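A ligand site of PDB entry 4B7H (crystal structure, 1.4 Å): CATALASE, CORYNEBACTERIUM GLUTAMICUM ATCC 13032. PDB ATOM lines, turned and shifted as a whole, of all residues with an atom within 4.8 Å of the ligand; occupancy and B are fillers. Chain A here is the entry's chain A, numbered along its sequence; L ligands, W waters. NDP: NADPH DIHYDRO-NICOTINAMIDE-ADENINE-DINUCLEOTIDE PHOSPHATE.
The backbone NH of Lys 300 lies close to the side-chain hydroxyl of Ser 298.
NH1 of Arg 197 lies within hydrogen-bond range of OH of Tyr 192 (3.1 Å).
A ring nitrogen (NE2) of His 229 lies within hydrogen-bond range of the side-chain amide oxygen (OE1) of Gln 276, 2.9 Å away.
OE1 of Gln 455 lies close to ND1 of His 188, at 3.1 Å.
OE1 of Gln 455 lies within hydrogen-bond range of N of Thr 296.
The backbone carbonyl oxygen (O) of Trp 297 sits at hydrogen-bond distance from the side-chain amide nitrogen (NE2) of Gln 276 (3.0 Å).
The backbone carbonyl oxygen of Leu 459 lies within hydrogen-bond range of the backbone NH of Leu 464 (3.0 Å).
NH2 of Arg 197 is in hydrogen-bond range of O2B of the ligand (3.2 Å).
The backbone NH of Gln 299 sits at hydrogen-bond distance from an oxygen (O1N) of the ligand (2.9 Å).
NE2 of His 188 sits at hydrogen-bond distance from O2D of the ligand, 2.7 Å away.
The side-chain hydroxyl (OG) of Ser 298 sits at hydrogen-bond distance from an oxygen (O2N) of the ligand (2.6 Å).
The side-chain amide oxygen (OE1) of Gln 299 sits close to an oxygen (O1N) of the ligand (3.0 Å).
The backbone carbonyl oxygen of Trp 297 lies within hydrogen-bond range of a nitrogen (N7N) of the ligand, at 2.9 Å.
OE2 of Glu 468 lies within hydrogen-bond range of N6A of the ligand, at 3.0 Å.
The backbone carbonyl oxygen (O) of Gln 455 lies within hydrogen-bond range of an oxygen (O3D) of the ligand (3.1 Å).
Water W8 lies within hydrogen-bond range of O3X of the ligand (2.6 Å), NZ of Lys 231 (3.1 Å) and NH2 of Arg 197 (3.3 Å).
Water W3 lies within hydrogen-bond range of an oxygen (O7N) of the ligand (2.7 Å), the side-chain amide oxygen of Gln 276 (2.8 Å) and the backbone NH of Trp 297 (3.1 Å).
Water W9 bridges an oxygen (O2X) of the ligand (2.7 Å) and the side-chain amino group (NZ) of Lys 231 (2.9 Å).
Water W5 lies within hydrogen-bond range of O of Tyr 192 (2.8 Å), N1A of the ligand (2.9 Å), N of Arg 197 (3.1 Å) and N of Asp 196 (3.4 Å).
Water W2 lies within hydrogen-bond range of the guanidinium group (NH1) of Arg 197 (2.9 Å), an oxygen (O3B) of the ligand (3.0 Å) and the side-chain amino group (NZ) of Lys 231 (3.3 Å).
Water W1 bridges N6A of the ligand (3.1 Å) and N of Asp 196 (3.3 Å).
CG of Pro 145 touches C4N of the ligand, 3.6 Å away.
Tyr 192 touches the ligand (CE2 to C2A, 3.5 Å).
His 229 touches the ligand.
Thr 296 touches the ligand (CB to N7N, 3.7 Å).
Leu 459 touches the ligand (CB to O2D, 3.5 Å).
Val 463 touches the ligand (CG1 to O4B, 3.7 Å).
Leu 464 touches the ligand.
Hydrophobic or aromatic side chains within 4 Å of the ligand: Pro 145, His 188, Tyr 192, His 229, Leu 459, Val 463 and Leu 464.
14 residues have an atom within 4 Å of the ligand: Pro 145, His 188, Tyr 192, Arg 197, His 229, Thr 296, Trp 297, Ser 298, Gln 299, Gln 455, Leu 459, Val 463, Leu 464 and Glu 468.
Along chain A the residues within 4 Å of the ligand span positions 145 to 468.
The nearest printed residue that does not touch the ligand is Gln 276 (4.1 Å).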
ATOM      1  N   PRO A 145      11.529 -27.618  -0.315  1.00  0.00           N
ATOM      2  CA  PRO A 145      11.115 -26.666  -1.355  1.00  0.00           C
ATOM      3  C   PRO A 145      12.307 -25.872  -1.921  1.00  0.00           C
ATOM      4  O   PRO A 145      12.127 -25.088  -2.856  1.00  0.00           O
ATOM      5  CB  PRO A 145      10.182 -25.718  -0.592  1.00  0.00           C
ATOM      6  CG  PRO A 145      10.789 -25.701   0.793  1.00  0.00           C
ATOM      7  CD  PRO A 145      11.142 -27.158   1.021  1.00  0.00           C
ATOM      8  N   HIS A 188      19.895 -21.463   3.640  1.00  0.00           N
ATOM      9  CA  HIS A 188      18.480 -21.804   3.671  1.00  0.00           C
ATOM     10  C   HIS A 188      18.278 -23.307   3.809  1.00  0.00           C
ATOM     11  O   HIS A 188      17.584 -23.765   4.724  1.00  0.00           O
ATOM     12  CB  HIS A 188      17.748 -21.281   2.429  1.00  0.00           C
ATOM     13  CG  HIS A 188      16.259 -21.263   2.581  1.00  0.00           C
ATOM     14  ND1 HIS A 188      15.406 -20.792   1.610  1.00  0.00           N
ATOM     15  CD2 HIS A 188      15.461 -21.673   3.607  1.00  0.00           C
ATOM     16  CE1 HIS A 188      14.157 -20.909   2.017  1.00  0.00           C
ATOM     17  NE2 HIS A 188      14.166 -21.429   3.232  1.00  0.00           N
ATOM     18  N   TYR A 192      16.943 -25.977   6.963  1.00  0.00           N
ATOM     19  CA  TYR A 192      15.888 -26.974   6.761  1.00  0.00           C
ATOM     20  C   TYR A 192      16.397 -28.387   7.107  1.00  0.00           C
ATOM     21  O   TYR A 192      15.722 -29.162   7.800  1.00  0.00           O
ATOM     22  CB  TYR A 192      15.413 -26.892   5.315  1.00  0.00           C
ATOM     23  CG  TYR A 192      14.155 -27.649   4.938  1.00  0.00           C
ATOM     24  CD1 TYR A 192      14.193 -29.003   4.639  1.00  0.00           C
ATOM     25  CD2 TYR A 192      12.941 -26.980   4.807  1.00  0.00           C
ATOM     26  CE1 TYR A 192      13.053 -29.692   4.259  1.00  0.00           C
ATOM     27  CE2 TYR A 192      11.788 -27.654   4.413  1.00  0.00           C
ATOM     28  CZ  TYR A 192      11.856 -29.012   4.140  1.00  0.00           C
ATOM     29  OH  TYR A 192      10.713 -29.672   3.752  1.00  0.00           O
ATOM     30  N   ASP A 196      13.913 -30.746  12.188  1.00  0.00           N
ATOM     31  CA  ASP A 196      13.247 -32.036  12.309  1.00  0.00           C
ATOM     32  C   ASP A 196      13.173 -32.755  10.961  1.00  0.00           C
ATOM     33  O   ASP A 196      13.264 -33.981  10.910  1.00  0.00           O
ATOM     34  CB  ASP A 196      11.826 -31.879  12.862  1.00  0.00           C
ATOM     35  CG  ASP A 196      11.779 -31.388  14.285  1.00  0.00           C
ATOM     36  OD1 ASP A 196      12.819 -31.374  14.990  1.00  0.00           O
ATOM     37  OD2 ASP A 196      10.676 -31.033  14.730  1.00  0.00           O
ATOM     38  N   ARG A 197      12.991 -31.997   9.887  1.00  0.00           N
ATOM     39  CA  ARG A 197      12.765 -32.585   8.564  1.00  0.00           C
ATOM     40  C   ARG A 197      13.996 -33.252   7.943  1.00  0.00           C
ATOM     41  O   ARG A 197      13.890 -33.935   6.926  1.00  0.00           O
ATOM     42  CB  ARG A 197      12.162 -31.572   7.596  1.00  0.00           C
ATOM     43  CG  ARG A 197      10.787 -31.104   8.034  1.00  0.00           C
ATOM     44  CD  ARG A 197      10.126 -30.272   6.970  1.00  0.00           C
ATOM     45  NE  ARG A 197       8.809 -29.840   7.427  1.00  0.00           N
ATOM     46  CZ  ARG A 197       7.934 -29.216   6.655  1.00  0.00           C
ATOM     47  NH1 ARG A 197       8.231 -28.960   5.388  1.00  0.00           N
ATOM     48  NH2 ARG A 197       6.767 -28.864   7.158  1.00  0.00           N
ATOM     49  N   PHE A 209       8.525 -31.865  -3.301  1.00  0.00           N
ATOM     50  CA  PHE A 209       8.497 -30.566  -3.985  1.00  0.00           C
ATOM     51  C   PHE A 209       9.276 -30.656  -5.273  1.00  0.00           C
ATOM     52  O   PHE A 209      10.263 -31.389  -5.334  1.00  0.00           O
ATOM     53  CB  PHE A 209       9.181 -29.483  -3.131  1.00  0.00           C
ATOM     54  CG  PHE A 209       8.622 -29.352  -1.738  1.00  0.00           C
ATOM     55  CD1 PHE A 209       9.111 -30.145  -0.715  1.00  0.00           C
ATOM     56  CD2 PHE A 209       7.643 -28.413  -1.443  1.00  0.00           C
ATOM     57  CE1 PHE A 209       8.622 -30.035   0.581  1.00  0.00           C
ATOM     58  CE2 PHE A 209       7.145 -28.280  -0.148  1.00  0.00           C
ATOM     59  CZ  PHE A 209       7.635 -29.094   0.870  1.00  0.00           C
ATOM     60  N   HIS A 229       4.099 -28.726  -5.324  1.00  0.00           N
ATOM     61  CA  HIS A 229       4.058 -29.169  -3.949  1.00  0.00           C
ATOM     62  C   HIS A 229       3.258 -30.446  -3.841  1.00  0.00           C
ATOM     63  O   HIS A 229       2.141 -30.504  -4.296  1.00  0.00           O
ATOM     64  CB  HIS A 229       3.423 -28.061  -3.032  1.00  0.00           C
ATOM     65  CG  HIS A 229       4.209 -26.784  -2.956  1.00  0.00           C
ATOM     66  ND1 HIS A 229       4.793 -26.365  -1.853  1.00  0.00           N
ATOM     67  CD2 HIS A 229       4.432 -25.839  -3.902  1.00  0.00           C
ATOM     68  CE1 HIS A 229       5.379 -25.238  -2.090  1.00  0.00           C
ATOM     69  NE2 HIS A 229       5.140 -24.899  -3.341  1.00  0.00           N
ATOM     70  N   LYS A 231       1.727 -32.749  -1.129  1.00  0.00           N
ATOM     71  CA  LYS A 231       1.447 -32.638   0.308  1.00  0.00           C
ATOM     72  C   LYS A 231       0.991 -33.981   0.869  1.00  0.00           C
ATOM     73  O   LYS A 231      -0.057 -34.514   0.466  1.00  0.00           O
ATOM     74  CB  LYS A 231       0.412 -31.533   0.585  1.00  0.00           C
ATOM     75  CG  LYS A 231       0.777 -30.163  -0.020  1.00  0.00           C
ATOM     76  CD  LYS A 231       2.062 -29.589   0.559  1.00  0.00           C
ATOM     77  CE  LYS A 231       1.900 -29.223   2.036  1.00  0.00           C
ATOM     78  NZ  LYS A 231       3.126 -28.527   2.563  1.00  0.00           N
ATOM     79  N   GLN A 276       1.962 -23.601  -6.771  1.00  0.00           N
ATOM     80  CA  GLN A 276       1.940 -22.149  -6.690  1.00  0.00           C
ATOM     81  C   GLN A 276       2.020 -21.642  -8.117  1.00  0.00           C
ATOM     82  O   GLN A 276       2.759 -22.183  -8.935  1.00  0.00           O
ATOM     83  CB  GLN A 276       3.149 -21.614  -5.907  1.00  0.00           C
ATOM     84  CG  GLN A 276       3.174 -22.007  -4.447  1.00  0.00           C
ATOM     85  CD  GLN A 276       4.438 -21.555  -3.754  1.00  0.00           C
ATOM     86  OE1 GLN A 276       5.500 -22.119  -3.984  1.00  0.00           O
ATOM     87  NE2 GLN A 276       4.319 -20.543  -2.907  1.00  0.00           N
ATOM     88  N   THR A 296      12.469 -19.647  -1.675  1.00  0.00           N
ATOM     89  CA  THR A 296      11.094 -20.114  -1.814  1.00  0.00           C
ATOM     90  C   THR A 296      10.168 -18.945  -2.129  1.00  0.00           C
ATOM     91  O   THR A 296      10.488 -17.788  -1.811  1.00  0.00           O
ATOM     92  CB  THR A 296      10.603 -20.843  -0.560  1.00  0.00           C
ATOM     93  OG1 THR A 296      10.872 -20.044   0.606  1.00  0.00           O
ATOM     94  CG2 THR A 296      11.304 -22.183  -0.410  1.00  0.00           C
ATOM     95  N   TRP A 297       9.031 -19.228  -2.760  1.00  0.00           N
ATOM     96  CA  TRP A 297       7.972 -18.233  -2.916  1.00  0.00           C
ATOM     97  C   TRP A 297       7.092 -18.338  -1.692  1.00  0.00           C
ATOM     98  O   TRP A 297       6.582 -19.423  -1.369  1.00  0.00           O
ATOM     99  CB  TRP A 297       7.095 -18.546  -4.126  1.00  0.00           C
ATOM    100  CG  TRP A 297       7.728 -18.487  -5.486  1.00  0.00           C
ATOM    101  CD1 TRP A 297       8.980 -18.024  -5.816  1.00  0.00           C
ATOM    102  CD2 TRP A 297       7.118 -18.914  -6.712  1.00  0.00           C
ATOM    103  NE1 TRP A 297       9.180 -18.142  -7.179  1.00  0.00           N
ATOM    104  CE2 TRP A 297       8.048 -18.682  -7.746  1.00  0.00           C
ATOM    105  CE3 TRP A 297       5.871 -19.477  -7.027  1.00  0.00           C
ATOM    106  CZ2 TRP A 297       7.768 -18.997  -9.075  1.00  0.00           C
ATOM    107  CZ3 TRP A 297       5.603 -19.787  -8.355  1.00  0.00           C
ATOM    108  CH2 TRP A 297       6.546 -19.556  -9.359  1.00  0.00           C
ATOM    109  N   SER A 298       6.875 -17.222  -0.992  1.00  0.00           N
ATOM    110  CA  SER A 298       6.024 -17.254   0.179  1.00  0.00           C
ATOM    111  C   SER A 298       4.603 -17.720  -0.169  1.00  0.00           C
ATOM    112  O   SER A 298       4.018 -17.270  -1.161  1.00  0.00           O
ATOM    113  CB  SER A 298       5.965 -15.899   0.853  1.00  0.00           C
ATOM    114  OG  SER A 298       5.027 -15.921   1.911  1.00  0.00           O
ATOM    115  N   GLN A 299       4.070 -18.628   0.649  1.00  0.00           N
ATOM    116  CA  GLN A 299       2.712 -19.128   0.454  1.00  0.00           C
ATOM    117  C   GLN A 299       1.672 -18.090   0.850  1.00  0.00           C
ATOM    118  O   GLN A 299       0.477 -18.259   0.591  1.00  0.00           O
ATOM    119  CB  GLN A 299       2.523 -20.449   1.201  1.00  0.00           C
ATOM    120  CG  GLN A 299       3.398 -21.548   0.590  1.00  0.00           C
ATOM    121  CD  GLN A 299       3.653 -22.716   1.522  1.00  0.00           C
ATOM    122  OE1 GLN A 299       4.400 -22.591   2.502  1.00  0.00           O
ATOM    123  NE2 GLN A 299       3.058 -23.852   1.201  1.00  0.00           N
ATOM    124  N   LYS A 300       2.125 -17.001   1.479  1.00  0.00           N
ATOM    125  CA  LYS A 300       1.240 -15.869   1.739  1.00  0.00           C
ATOM    126  C   LYS A 300       1.062 -15.046   0.471  1.00  0.00           C
ATOM    127  O   LYS A 300       0.027 -14.414   0.282  1.00  0.00           O
ATOM    128  CB  LYS A 300       1.806 -15.003   2.865  1.00  0.00           C
ATOM    129  CG  LYS A 300       2.169 -15.769   4.113  1.00  0.00           C
ATOM    130  CD  LYS A 300       2.487 -14.842   5.271  1.00  0.00           C
ATOM    131  CE  LYS A 300       3.370 -15.517   6.301  1.00  0.00           C
ATOM    132  NZ  LYS A 300       3.446 -14.728   7.566  1.00  0.00           N
ATOM    133  N   GLN A 455      15.760 -15.823   4.423  1.00  0.00           N
ATOM    134  CA  GLN A 455      14.737 -16.861   4.423  1.00  0.00           C
ATOM    135  C   GLN A 455      14.875 -17.905   5.553  1.00  0.00           C
ATOM    136  O   GLN A 455      13.888 -18.226   6.197  1.00  0.00           O
ATOM    137  CB  GLN A 455      14.559 -17.502   3.038  1.00  0.00           C
ATOM    138  CG  GLN A 455      13.912 -16.541   2.022  1.00  0.00           C
ATOM    139  CD  GLN A 455      13.293 -17.265   0.855  1.00  0.00           C
ATOM    140  OE1 GLN A 455      13.663 -18.397   0.559  1.00  0.00           O
ATOM    141  NE2 GLN A 455      12.354 -16.635   0.188  1.00  0.00           N
ATOM    142  N   ILE A 458      13.752 -16.100   8.644  1.00  0.00           N
ATOM    143  CA  ILE A 458      12.295 -16.068   8.700  1.00  0.00           C
ATOM    144  C   ILE A 458      11.719 -17.403   9.185  1.00  0.00           C
ATOM    145  O   ILE A 458      10.802 -17.436  10.019  1.00  0.00           O
ATOM    146  CB  ILE A 458      11.695 -15.678   7.320  1.00  0.00           C
ATOM    147  CG1 ILE A 458      11.966 -14.205   7.021  1.00  0.00           C
ATOM    148  CG2 ILE A 458      10.199 -15.936   7.287  1.00  0.00           C
ATOM    149  CD1 ILE A 458      11.597 -13.779   5.609  1.00  0.00           C
ATOM    150  N   LEU A 459      12.248 -18.510   8.665  1.00  0.00           N
ATOM    151  CA  LEU A 459      11.834 -19.827   9.135  1.00  0.00           C
ATOM    152  C   LEU A 459      12.029 -19.929  10.655  1.00  0.00           C
ATOM    153  O   LEU A 459      11.115 -20.317  11.373  1.00  0.00           O
ATOM    154  CB  LEU A 459      12.620 -20.930   8.412  1.00  0.00           C
ATOM    155  CG  LEU A 459      12.456 -22.394   8.848  1.00  0.00           C
ATOM    156  CD1 LEU A 459      11.016 -22.872   8.720  1.00  0.00           C
ATOM    157  CD2 LEU A 459      13.386 -23.307   8.048  1.00  0.00           C
ATOM    158  N   VAL A 463       8.255 -19.098  11.818  1.00  0.00           N
ATOM    159  CA  VAL A 463       7.589 -20.366  11.514  1.00  0.00           C
ATOM    160  C   VAL A 463       7.787 -21.435  12.587  1.00  0.00           C
ATOM    161  O   VAL A 463       6.816 -22.021  13.082  1.00  0.00           O
ATOM    162  CB  VAL A 463       8.044 -20.938  10.161  1.00  0.00           C
ATOM    163  CG1 VAL A 463       7.425 -22.318   9.925  1.00  0.00           C
ATOM    164  CG2 VAL A 463       7.707 -19.986   9.017  1.00  0.00           C
ATOM    165  N   LEU A 464       9.039 -21.737  12.925  1.00  0.00           N
ATOM    166  CA  LEU A 464       9.328 -22.817  13.861  1.00  0.00           C
ATOM    167  C   LEU A 464       8.744 -22.561  15.241  1.00  0.00           C
ATOM    168  O   LEU A 464       8.738 -21.420  15.733  1.00  0.00           O
ATOM    169  CB  LEU A 464      10.836 -23.015  13.998  1.00  0.00           C
ATOM    170  CG  LEU A 464      11.589 -23.394  12.727  1.00  0.00           C
ATOM    171  CD1 LEU A 464      13.045 -23.670  13.066  1.00  0.00           C
ATOM    172  CD2 LEU A 464      10.956 -24.594  12.028  1.00  0.00           C
ATOM    173  N   GLU A 468      10.988 -26.909  17.990  1.00  0.00           N
ATOM    174  CA  GLU A 468      11.722 -26.991  16.739  1.00  0.00           C
ATOM    175  C   GLU A 468      12.974 -26.130  16.756  1.00  0.00           C
ATOM    176  O   GLU A 468      14.028 -26.550  16.281  1.00  0.00           O
ATOM    177  CB  GLU A 468      10.814 -26.611  15.557  1.00  0.00           C
ATOM    178  CG  GLU A 468       9.706 -27.617  15.293  1.00  0.00           C
ATOM    179  CD  GLU A 468       8.711 -27.140  14.256  1.00  0.00           C
ATOM    180  OE1 GLU A 468       8.307 -25.953  14.309  1.00  0.00           O
ATOM    181  OE2 GLU A 468       8.300 -27.943  13.374  1.00  0.00           O
HETATM  182  PA  NDP L   1       4.145 -20.074   5.617  1.00  0.00           P
HETATM  183  O1A NDP L   1       3.780 -19.921   7.050  1.00  0.00           O
HETATM  184  O2A NDP L   1       3.001 -19.842   4.699  1.00  0.00           O
HETATM  185  O5B NDP L   1       4.728 -21.551   5.409  1.00  0.00           O
HETATM  186  C5B NDP L   1       5.701 -22.058   6.283  1.00  0.00           C
HETATM  187  C4B NDP L   1       6.072 -23.442   5.766  1.00  0.00           C
HETATM  188  O4B NDP L   1       7.081 -23.992   6.593  1.00  0.00           O
HETATM  189  C3B NDP L   1       4.866 -24.387   5.792  1.00  0.00           C
HETATM  190  O3B NDP L   1       4.825 -25.143   4.599  1.00  0.00           O
HETATM  191  C2B NDP L   1       5.168 -25.245   7.004  1.00  0.00           C
HETATM  192  O2B NDP L   1       4.553 -26.525   7.007  1.00  0.00           O
HETATM  193  C1B NDP L   1       6.689 -25.302   6.932  1.00  0.00           C
HETATM  194  N9A NDP L   1       7.307 -25.843   8.163  1.00  0.00           N
HETATM  195  C8A NDP L   1       6.721 -26.035   9.389  1.00  0.00           C
HETATM  196  N7A NDP L   1       7.630 -26.584  10.224  1.00  0.00           N
HETATM  197  C5A NDP L   1       8.791 -26.755   9.556  1.00  0.00           C
HETATM  198  C6A NDP L   1      10.028 -27.276   9.927  1.00  0.00           C
HETATM  199  N6A NDP L   1      10.137 -28.008  11.027  1.00  0.00           N
HETATM  200  N1A NDP L   1      11.045 -27.304   9.000  1.00  0.00           N
HETATM  201  C2A NDP L   1      10.846 -26.851   7.718  1.00  0.00           C
HETATM  202  N3A NDP L   1       9.607 -26.344   7.348  1.00  0.00           N
HETATM  203  C4A NDP L   1       8.600 -26.296   8.251  1.00  0.00           C
HETATM  204  O3  NDP L   1       5.390 -19.079   5.308  1.00  0.00           O
HETATM  205  PN  NDP L   1       6.125 -18.917   3.876  1.00  0.00           P
HETATM  206  O1N NDP L   1       5.492 -19.805   2.855  1.00  0.00           O
HETATM  207  O2N NDP L   1       6.247 -17.461   3.639  1.00  0.00           O
HETATM  208  O5D NDP L   1       7.602 -19.470   4.166  1.00  0.00           O
HETATM  209  C5D NDP L   1       8.264 -19.152   5.379  1.00  0.00           C
HETATM  210  C4D NDP L   1       9.462 -20.060   5.555  1.00  0.00           C
HETATM  211  O4D NDP L   1       9.014 -21.392   5.634  1.00  0.00           O
HETATM  212  C3D NDP L   1      10.390 -19.984   4.348  1.00  0.00           C
HETATM  213  O3D NDP L   1      11.401 -19.009   4.535  1.00  0.00           O
HETATM  214  C2D NDP L   1      10.933 -21.401   4.256  1.00  0.00           C
HETATM  215  O2D NDP L   1      12.119 -21.495   4.991  1.00  0.00           O
HETATM  216  C1D NDP L   1       9.894 -22.279   4.956  1.00  0.00           C
HETATM  217  N1N NDP L   1       9.140 -23.104   3.990  1.00  0.00           N
HETATM  218  C2N NDP L   1       8.625 -22.517   2.876  1.00  0.00           C
HETATM  219  C3N NDP L   1       7.900 -23.224   1.925  1.00  0.00           C
HETATM  220  C7N NDP L   1       7.400 -22.486   0.725  1.00  0.00           C
HETATM  221  O7N NDP L   1       7.247 -23.188  -0.470  1.00  0.00           O
HETATM  222  N7N NDP L   1       7.135 -21.190   0.802  1.00  0.00           N
HETATM  223  C4N NDP L   1       7.619 -24.701   2.067  1.00  0.00           C
HETATM  224  C5N NDP L   1       8.224 -25.254   3.327  1.00  0.00           C
HETATM  225  C6N NDP L   1       8.937 -24.447   4.214  1.00  0.00           C
HETATM  226  P2B NDP L   1       3.144 -26.764   7.764  1.00  0.00           P
HETATM  227  O1X NDP L   1       3.310 -26.313   9.198  1.00  0.00           O
HETATM  228  O2X NDP L   1       2.091 -25.953   7.055  1.00  0.00           O
HETATM  229  O3X NDP L   1       2.844 -28.246   7.667  1.00  0.00           O
HETATM  230  O   HOH W   1      12.802 -27.714  12.583  1.00  0.00           O
HETATM  231  O   HOH W   2       5.930 -27.863   4.074  1.00  0.00           O
HETATM  232  O   HOH W   3       8.065 -22.144  -2.788  1.00  0.00           O
HETATM  233  O   HOH W   4       3.194 -30.458   9.074  1.00  0.00           O
HETATM  234  O   HOH W   5      13.395 -28.978   9.336  1.00  0.00           O
HETATM  235  O   HOH W   6      10.512 -16.698   3.196  1.00  0.00           O
HETATM  236  O   HOH W   7       8.208 -15.446   4.184  1.00  0.00           O
HETATM  237  O   HOH W   8       3.927 -29.228   5.473  1.00  0.00           O
HETATM  238  O   HOH W   9       2.356 -26.374   4.382  1.00  0.00           O
HETATM  239  O   HOH W  10       4.619 -27.575  11.322  1.00  0.00           O
HETATM  240  O   HOH W  11       1.347 -22.195   4.686  1.00  0.00           O
